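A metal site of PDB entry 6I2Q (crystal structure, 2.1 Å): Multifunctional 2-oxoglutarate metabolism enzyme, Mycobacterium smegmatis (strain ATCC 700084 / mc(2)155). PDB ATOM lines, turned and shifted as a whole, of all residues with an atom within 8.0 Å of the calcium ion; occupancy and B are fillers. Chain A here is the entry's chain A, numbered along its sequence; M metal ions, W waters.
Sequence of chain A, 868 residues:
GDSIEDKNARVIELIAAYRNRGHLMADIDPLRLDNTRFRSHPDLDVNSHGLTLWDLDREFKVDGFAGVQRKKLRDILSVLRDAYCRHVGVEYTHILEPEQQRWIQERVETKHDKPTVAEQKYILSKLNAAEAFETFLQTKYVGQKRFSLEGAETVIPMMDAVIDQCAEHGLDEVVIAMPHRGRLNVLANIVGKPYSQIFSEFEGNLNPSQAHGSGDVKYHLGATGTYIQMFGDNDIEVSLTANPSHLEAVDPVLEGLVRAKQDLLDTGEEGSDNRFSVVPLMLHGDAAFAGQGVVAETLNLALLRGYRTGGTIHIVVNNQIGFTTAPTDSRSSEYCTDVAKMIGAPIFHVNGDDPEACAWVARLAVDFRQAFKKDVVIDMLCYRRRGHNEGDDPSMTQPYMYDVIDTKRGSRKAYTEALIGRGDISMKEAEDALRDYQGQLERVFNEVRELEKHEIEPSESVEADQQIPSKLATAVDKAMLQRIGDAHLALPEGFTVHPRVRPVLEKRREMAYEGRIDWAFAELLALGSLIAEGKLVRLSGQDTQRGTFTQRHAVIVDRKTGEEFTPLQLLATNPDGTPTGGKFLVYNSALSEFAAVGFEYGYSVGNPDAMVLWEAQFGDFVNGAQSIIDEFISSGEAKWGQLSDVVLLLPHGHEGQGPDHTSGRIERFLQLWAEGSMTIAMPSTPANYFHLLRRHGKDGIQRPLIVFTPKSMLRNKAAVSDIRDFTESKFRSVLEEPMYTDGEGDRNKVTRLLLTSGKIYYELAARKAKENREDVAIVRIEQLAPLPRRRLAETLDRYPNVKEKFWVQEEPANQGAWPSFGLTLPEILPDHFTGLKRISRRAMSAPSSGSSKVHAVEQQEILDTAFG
The backbone NH of Arg 703 sits close to the side-chain carboxylate of Asp 645, 3.0 Å away.
The calcium ion is bound by the backbone carbonyl oxygen (O) of Ile 701 (2.2 Å), the backbone carbonyl oxygen (O) of His 696 (2.2 Å), water W2 (2.4 Å), the side-chain carboxylate (OD2) of Asp 699 (2.5 Å), water W1 (2.5 Å), the side-chain carboxylate (OD2) of Asp 645 (2.6 Å) and the side-chain carboxylate (OD1) of Asp 645 (2.6 Å). The calcium ion has seven donor atoms within binding distance.
Water W2 lies within hydrogen-bond range of OD1 of Asp 699 (2.7 Å) and ND1 of His 696 (3.0 Å).
Of the 23 residues printed, 4 come within 4 Å of the calcium ion. The nearest printed residue that does not touch the calcium ion is Gln 702 (4.4 Å).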
ATOM      1  N   LYS A 535     -33.687  13.849  -9.044  1.00  0.00           N
ATOM      2  CA  LYS A 535     -33.775  15.247  -9.411  1.00  0.00           C
ATOM      3  C   LYS A 535     -33.617  15.473 -10.912  1.00  0.00           C
ATOM      4  O   LYS A 535     -32.817  14.811 -11.584  1.00  0.00           O
ATOM      5  CB  LYS A 535     -32.726  16.071  -8.650  1.00  0.00           C
ATOM      6  CG  LYS A 535     -33.238  17.447  -8.270  1.00  0.00           C
ATOM      7  CD  LYS A 535     -32.179  18.314  -7.604  1.00  0.00           C
ATOM      8  CE  LYS A 535     -32.664  19.746  -7.391  1.00  0.00           C
ATOM      9  NZ  LYS A 535     -33.891  19.822  -6.537  1.00  0.00           N
ATOM     10  N   PRO A 608     -39.406  24.812  -9.360  1.00  0.00           N
ATOM     11  CA  PRO A 608     -38.510  24.990  -8.198  1.00  0.00           C
ATOM     12  C   PRO A 608     -37.742  23.725  -7.792  1.00  0.00           C
ATOM     13  O   PRO A 608     -36.708  23.832  -7.100  1.00  0.00           O
ATOM     14  CB  PRO A 608     -39.457  25.403  -7.053  1.00  0.00           C
ATOM     15  CG  PRO A 608     -40.663  25.950  -7.747  1.00  0.00           C
ATOM     16  CD  PRO A 608     -40.817  25.125  -8.999  1.00  0.00           C
ATOM     17  N   ALA A 610     -36.234  21.647  -9.976  1.00  0.00           N
ATOM     18  CA  ALA A 610     -35.168  21.324 -10.904  1.00  0.00           C
ATOM     19  C   ALA A 610     -33.852  21.966 -10.445  1.00  0.00           C
ATOM     20  O   ALA A 610     -33.860  22.989  -9.769  1.00  0.00           O
ATOM     21  CB  ALA A 610     -35.537  21.804 -12.308  1.00  0.00           C
ATOM     22  N   MET A 611     -32.719  21.331 -10.778  1.00  0.00           N
ATOM     23  CA  MET A 611     -31.353  21.857 -10.629  1.00  0.00           C
ATOM     24  C   MET A 611     -31.073  22.539 -11.982  1.00  0.00           C
ATOM     25  O   MET A 611     -31.101  21.857 -13.013  1.00  0.00           O
ATOM     26  CB  MET A 611     -30.359  20.731 -10.294  1.00  0.00           C
ATOM     27  CG  MET A 611     -28.924  21.215 -10.067  1.00  0.00           C
ATOM     28  SD  MET A 611     -28.632  21.908  -8.426  1.00  0.00           S
ATOM     29  CE  MET A 611     -26.897  22.322  -8.546  1.00  0.00           C
ATOM     30  N   SER A 644     -36.114  31.999  -7.236  1.00  0.00           N
ATOM     31  CA  SER A 644     -35.357  31.267  -8.249  1.00  0.00           C
ATOM     32  C   SER A 644     -34.145  30.599  -7.633  1.00  0.00           C
ATOM     33  O   SER A 644     -33.464  31.183  -6.793  1.00  0.00           O
ATOM     34  CB  SER A 644     -34.921  32.210  -9.356  1.00  0.00           C
ATOM     35  OG  SER A 644     -34.079  31.547 -10.292  1.00  0.00           O
ATOM     36  N   ASP A 645     -33.853  29.382  -8.075  1.00  0.00           N
ATOM     37  CA  ASP A 645     -32.718  28.593  -7.632  1.00  0.00           C
ATOM     38  C   ASP A 645     -31.701  28.465  -8.745  1.00  0.00           C
ATOM     39  O   ASP A 645     -30.890  27.544  -8.711  1.00  0.00           O
ATOM     40  CB  ASP A 645     -33.178  27.199  -7.176  1.00  0.00           C
ATOM     41  CG  ASP A 645     -32.360  26.670  -6.006  1.00  0.00           C
ATOM     42  OD1 ASP A 645     -31.952  27.483  -5.150  1.00  0.00           O
ATOM     43  OD2 ASP A 645     -32.136  25.443  -5.961  1.00  0.00           O
ATOM     44  N   VAL A 646     -31.695  29.391  -9.727  1.00  0.00           N
ATOM     45  CA  VAL A 646     -30.773  29.287 -10.865  1.00  0.00           C
ATOM     46  C   VAL A 646     -29.272  29.387 -10.427  1.00  0.00           C
ATOM     47  O   VAL A 646     -28.930  30.136  -9.508  1.00  0.00           O
ATOM     48  CB  VAL A 646     -31.136  30.298 -11.998  1.00  0.00           C
ATOM     49  CG1 VAL A 646     -30.911  31.744 -11.570  1.00  0.00           C
ATOM     50  CG2 VAL A 646     -30.428  29.980 -13.306  1.00  0.00           C
ATOM     51  N   VAL A 647     -28.419  28.613 -11.087  1.00  0.00           N
ATOM     52  CA  VAL A 647     -26.973  28.633 -10.866  1.00  0.00           C
ATOM     53  C   VAL A 647     -26.324  29.294 -12.074  1.00  0.00           C
ATOM     54  O   VAL A 647     -26.613  28.890 -13.197  1.00  0.00           O
ATOM     55  CB  VAL A 647     -26.357  27.219 -10.610  1.00  0.00           C
ATOM     56  CG1 VAL A 647     -24.843  27.310 -10.328  1.00  0.00           C
ATOM     57  CG2 VAL A 647     -27.065  26.475  -9.491  1.00  0.00           C
ATOM     58  N   THR A 679     -26.272  33.366  -3.099  1.00  0.00           N
ATOM     59  CA  THR A 679     -25.085  32.730  -2.571  1.00  0.00           C
ATOM     60  C   THR A 679     -24.028  32.926  -3.645  1.00  0.00           C
ATOM     61  O   THR A 679     -24.295  32.709  -4.838  1.00  0.00           O
ATOM     62  CB  THR A 679     -25.303  31.245  -2.184  1.00  0.00           C
ATOM     63  OG1 THR A 679     -26.419  31.110  -1.301  1.00  0.00           O
ATOM     64  CG2 THR A 679     -24.070  30.631  -1.523  1.00  0.00           C
ATOM     65  N   LEU A 692     -20.982  22.023  -2.581  1.00  0.00           N
ATOM     66  CA  LEU A 692     -21.679  23.281  -2.872  1.00  0.00           C
ATOM     67  C   LEU A 692     -22.889  23.033  -3.772  1.00  0.00           C
ATOM     68  O   LEU A 692     -23.985  23.502  -3.464  1.00  0.00           O
ATOM     69  CB  LEU A 692     -20.718  24.286  -3.564  1.00  0.00           C
ATOM     70  CG  LEU A 692     -21.329  25.658  -3.905  1.00  0.00           C
ATOM     71  CD1 LEU A 692     -21.309  26.584  -2.711  1.00  0.00           C
ATOM     72  CD2 LEU A 692     -20.606  26.285  -5.085  1.00  0.00           C
ATOM     73  N   LEU A 693     -22.685  22.281  -4.872  1.00  0.00           N
ATOM     74  CA  LEU A 693     -23.763  21.975  -5.804  1.00  0.00           C
ATOM     75  C   LEU A 693     -24.829  21.104  -5.171  1.00  0.00           C
ATOM     76  O   LEU A 693     -26.004  21.352  -5.425  1.00  0.00           O
ATOM     77  CB  LEU A 693     -23.256  21.304  -7.094  1.00  0.00           C
ATOM     78  CG  LEU A 693     -22.414  22.129  -8.060  1.00  0.00           C
ATOM     79  CD1 LEU A 693     -22.083  21.298  -9.277  1.00  0.00           C
ATOM     80  CD2 LEU A 693     -23.158  23.390  -8.512  1.00  0.00           C
ATOM     81  N   ARG A 694     -24.432  20.068  -4.396  1.00  0.00           N
ATOM     82  CA  ARG A 694     -25.385  19.155  -3.765  1.00  0.00           C
ATOM     83  C   ARG A 694     -26.209  19.906  -2.710  1.00  0.00           C
ATOM     84  O   ARG A 694     -27.407  19.690  -2.631  1.00  0.00           O
ATOM     85  CB  ARG A 694     -24.706  17.914  -3.134  1.00  0.00           C
ATOM     86  CG  ARG A 694     -23.799  17.104  -4.056  1.00  0.00           C
ATOM     87  CD  ARG A 694     -24.302  15.721  -4.411  1.00  0.00           C
ATOM     88  NE  ARG A 694     -24.789  14.967  -3.255  1.00  0.00           N
ATOM     89  CZ  ARG A 694     -25.901  14.225  -3.288  1.00  0.00           C
ATOM     90  NH1 ARG A 694     -26.601  14.113  -4.407  1.00  0.00           N
ATOM     91  NH2 ARG A 694     -26.305  13.588  -2.204  1.00  0.00           N
ATOM     92  N   ARG A 695     -25.562  20.794  -1.927  1.00  0.00           N
ATOM     93  CA  ARG A 695     -26.252  21.617  -0.914  1.00  0.00           C
ATOM     94  C   ARG A 695     -27.292  22.483  -1.588  1.00  0.00           C
ATOM     95  O   ARG A 695     -28.437  22.496  -1.142  1.00  0.00           O
ATOM     96  CB  ARG A 695     -25.258  22.489  -0.112  1.00  0.00           C
ATOM     97  CG  ARG A 695     -25.945  23.382   0.929  1.00  0.00           C
ATOM     98  CD  ARG A 695     -24.975  24.258   1.684  1.00  0.00           C
ATOM     99  NE  ARG A 695     -24.376  25.307   0.848  1.00  0.00           N
ATOM    100  CZ  ARG A 695     -23.567  26.260   1.299  1.00  0.00           C
ATOM    101  NH1 ARG A 695     -23.239  26.298   2.585  1.00  0.00           N
ATOM    102  NH2 ARG A 695     -23.063  27.166   0.478  1.00  0.00           N
ATOM    103  N   HIS A 696     -26.911  23.164  -2.694  1.00  0.00           N
ATOM    104  CA  HIS A 696     -27.781  24.039  -3.470  1.00  0.00           C
ATOM    105  C   HIS A 696     -29.033  23.305  -3.986  1.00  0.00           C
ATOM    106  O   HIS A 696     -30.144  23.849  -3.908  1.00  0.00           O
ATOM    107  CB  HIS A 696     -27.026  24.651  -4.639  1.00  0.00           C
ATOM    108  CG  HIS A 696     -27.868  25.609  -5.428  1.00  0.00           C
ATOM    109  ND1 HIS A 696     -28.137  26.891  -4.967  1.00  0.00           N
ATOM    110  CD2 HIS A 696     -28.524  25.409  -6.595  1.00  0.00           C
ATOM    111  CE1 HIS A 696     -28.916  27.438  -5.883  1.00  0.00           C
ATOM    112  NE2 HIS A 696     -29.192  26.588  -6.870  1.00  0.00           N
ATOM    113  N   GLY A 697     -28.840  22.091  -4.493  1.00  0.00           N
ATOM    114  CA  GLY A 697     -29.943  21.282  -5.023  1.00  0.00           C
ATOM    115  C   GLY A 697     -30.781  20.587  -3.974  1.00  0.00           C
ATOM    116  O   GLY A 697     -31.924  20.184  -4.248  1.00  0.00           O
ATOM    117  N   LYS A 698     -30.246  20.429  -2.748  1.00  0.00           N
ATOM    118  CA  LYS A 698     -30.965  19.676  -1.725  1.00  0.00           C
ATOM    119  C   LYS A 698     -31.379  20.508  -0.512  1.00  0.00           C
ATOM    120  O   LYS A 698     -32.021  19.947   0.378  1.00  0.00           O
ATOM    121  CB  LYS A 698     -30.075  18.508  -1.245  1.00  0.00           C
ATOM    122  CG  LYS A 698     -29.820  17.454  -2.332  1.00  0.00           C
ATOM    123  CD  LYS A 698     -28.649  16.494  -1.993  1.00  0.00           C
ATOM    124  CE  LYS A 698     -28.952  15.475  -0.902  1.00  0.00           C
ATOM    125  NZ  LYS A 698     -30.132  14.627  -1.208  1.00  0.00           N
ATOM    126  N   ASP A 699     -31.028  21.795  -0.423  1.00  0.00           N
ATOM    127  CA  ASP A 699     -31.327  22.573   0.790  1.00  0.00           C
ATOM    128  C   ASP A 699     -32.824  22.959   0.970  1.00  0.00           C
ATOM    129  O   ASP A 699     -33.180  23.463   2.026  1.00  0.00           O
ATOM    130  CB  ASP A 699     -30.439  23.837   0.858  1.00  0.00           C
ATOM    131  CG  ASP A 699     -30.577  24.780  -0.330  1.00  0.00           C
ATOM    132  OD1 ASP A 699     -29.767  25.722  -0.431  1.00  0.00           O
ATOM    133  OD2 ASP A 699     -31.485  24.558  -1.175  1.00  0.00           O
ATOM    134  N   GLY A 700     -33.636  22.786  -0.065  1.00  0.00           N
ATOM    135  CA  GLY A 700     -35.054  23.184  -0.021  1.00  0.00           C
ATOM    136  C   GLY A 700     -35.245  24.692   0.031  1.00  0.00           C
ATOM    137  O   GLY A 700     -36.271  25.175   0.530  1.00  0.00           O
ATOM    138  N   ILE A 701     -34.239  25.448  -0.415  1.00  0.00           N
ATOM    139  CA  ILE A 701     -34.232  26.905  -0.465  1.00  0.00           C
ATOM    140  C   ILE A 701     -34.090  27.277  -1.948  1.00  0.00           C
ATOM    141  O   ILE A 701     -33.317  26.637  -2.680  1.00  0.00           O
ATOM    142  CB  ILE A 701     -33.112  27.526   0.448  1.00  0.00           C
ATOM    143  CG1 ILE A 701     -33.454  27.338   1.955  1.00  0.00           C
ATOM    144  CG2 ILE A 701     -32.825  29.028   0.148  1.00  0.00           C
ATOM    145  CD1 ILE A 701     -32.255  27.404   2.905  1.00  0.00           C
ATOM    146  N   GLN A 702     -34.856  28.276  -2.382  1.00  0.00           N
ATOM    147  CA  GLN A 702     -34.852  28.820  -3.742  1.00  0.00           C
ATOM    148  C   GLN A 702     -34.104  30.143  -3.673  1.00  0.00           C
ATOM    149  O   GLN A 702     -34.657  31.155  -3.217  1.00  0.00           O
ATOM    150  CB  GLN A 702     -36.286  28.962  -4.309  1.00  0.00           C
ATOM    151  CG  GLN A 702     -37.156  27.691  -4.211  1.00  0.00           C
ATOM    152  CD  GLN A 702     -36.498  26.481  -4.824  1.00  0.00           C
ATOM    153  OE1 GLN A 702     -36.253  26.438  -6.015  1.00  0.00           O
ATOM    154  NE2 GLN A 702     -36.180  25.468  -4.013  1.00  0.00           N
ATOM    155  N   ARG A 703     -32.818  30.107  -4.037  1.00  0.00           N
ATOM    156  CA  ARG A 703     -31.927  31.255  -3.977  1.00  0.00           C
ATOM    157  C   ARG A 703     -30.845  31.082  -5.020  1.00  0.00           C
ATOM    158  O   ARG A 703     -30.235  30.009  -5.064  1.00  0.00           O
ATOM    159  CB  ARG A 703     -31.317  31.399  -2.575  1.00  0.00           C
ATOM    160  CG  ARG A 703     -30.415  32.616  -2.411  1.00  0.00           C
ATOM    161  CD  ARG A 703     -30.000  32.808  -0.977  1.00  0.00           C
ATOM    162  NE  ARG A 703     -31.188  32.892  -0.111  1.00  0.00           N
ATOM    163  CZ  ARG A 703     -31.190  32.619   1.182  1.00  0.00           C
ATOM    164  NH1 ARG A 703     -30.062  32.272   1.798  1.00  0.00           N
ATOM    165  NH2 ARG A 703     -32.315  32.692   1.879  1.00  0.00           N
ATOM    166  N   PRO A 704     -30.599  32.085  -5.892  1.00  0.00           N
ATOM    167  CA  PRO A 704     -29.564  31.901  -6.919  1.00  0.00           C
ATOM    168  C   PRO A 704     -28.158  31.712  -6.349  1.00  0.00           C
ATOM    169  O   PRO A 704     -27.820  32.257  -5.297  1.00  0.00           O
ATOM    170  CB  PRO A 704     -29.651  33.194  -7.746  1.00  0.00           C
ATOM    171  CG  PRO A 704     -31.017  33.740  -7.466  1.00  0.00           C
ATOM    172  CD  PRO A 704     -31.244  33.408  -6.018  1.00  0.00           C
ATOM    173  N   LEU A 705     -27.376  30.909  -7.069  1.00  0.00           N
ATOM    174  CA  LEU A 705     -25.991  30.620  -6.729  1.00  0.00           C
ATOM    175  C   LEU A 705     -25.084  31.116  -7.868  1.00  0.00           C
ATOM    176  O   LEU A 705     -25.323  30.779  -9.024  1.00  0.00           O
ATOM    177  CB  LEU A 705     -25.794  29.101  -6.459  1.00  0.00           C
ATOM    178  CG  LEU A 705     -24.342  28.562  -6.381  1.00  0.00           C
ATOM    179  CD1 LEU A 705     -23.527  29.219  -5.225  1.00  0.00           C
ATOM    180  CD2 LEU A 705     -24.327  27.026  -6.300  1.00  0.00           C
HETATM  181 CA    CA M   1     -31.585  25.500  -3.456  1.00  0.00          CA
HETATM  182  O   HOH W   1     -33.370  23.696  -3.627  1.00  0.00           O
HETATM  183  O   HOH W   2     -30.016  27.166  -2.643  1.00  0.00           O
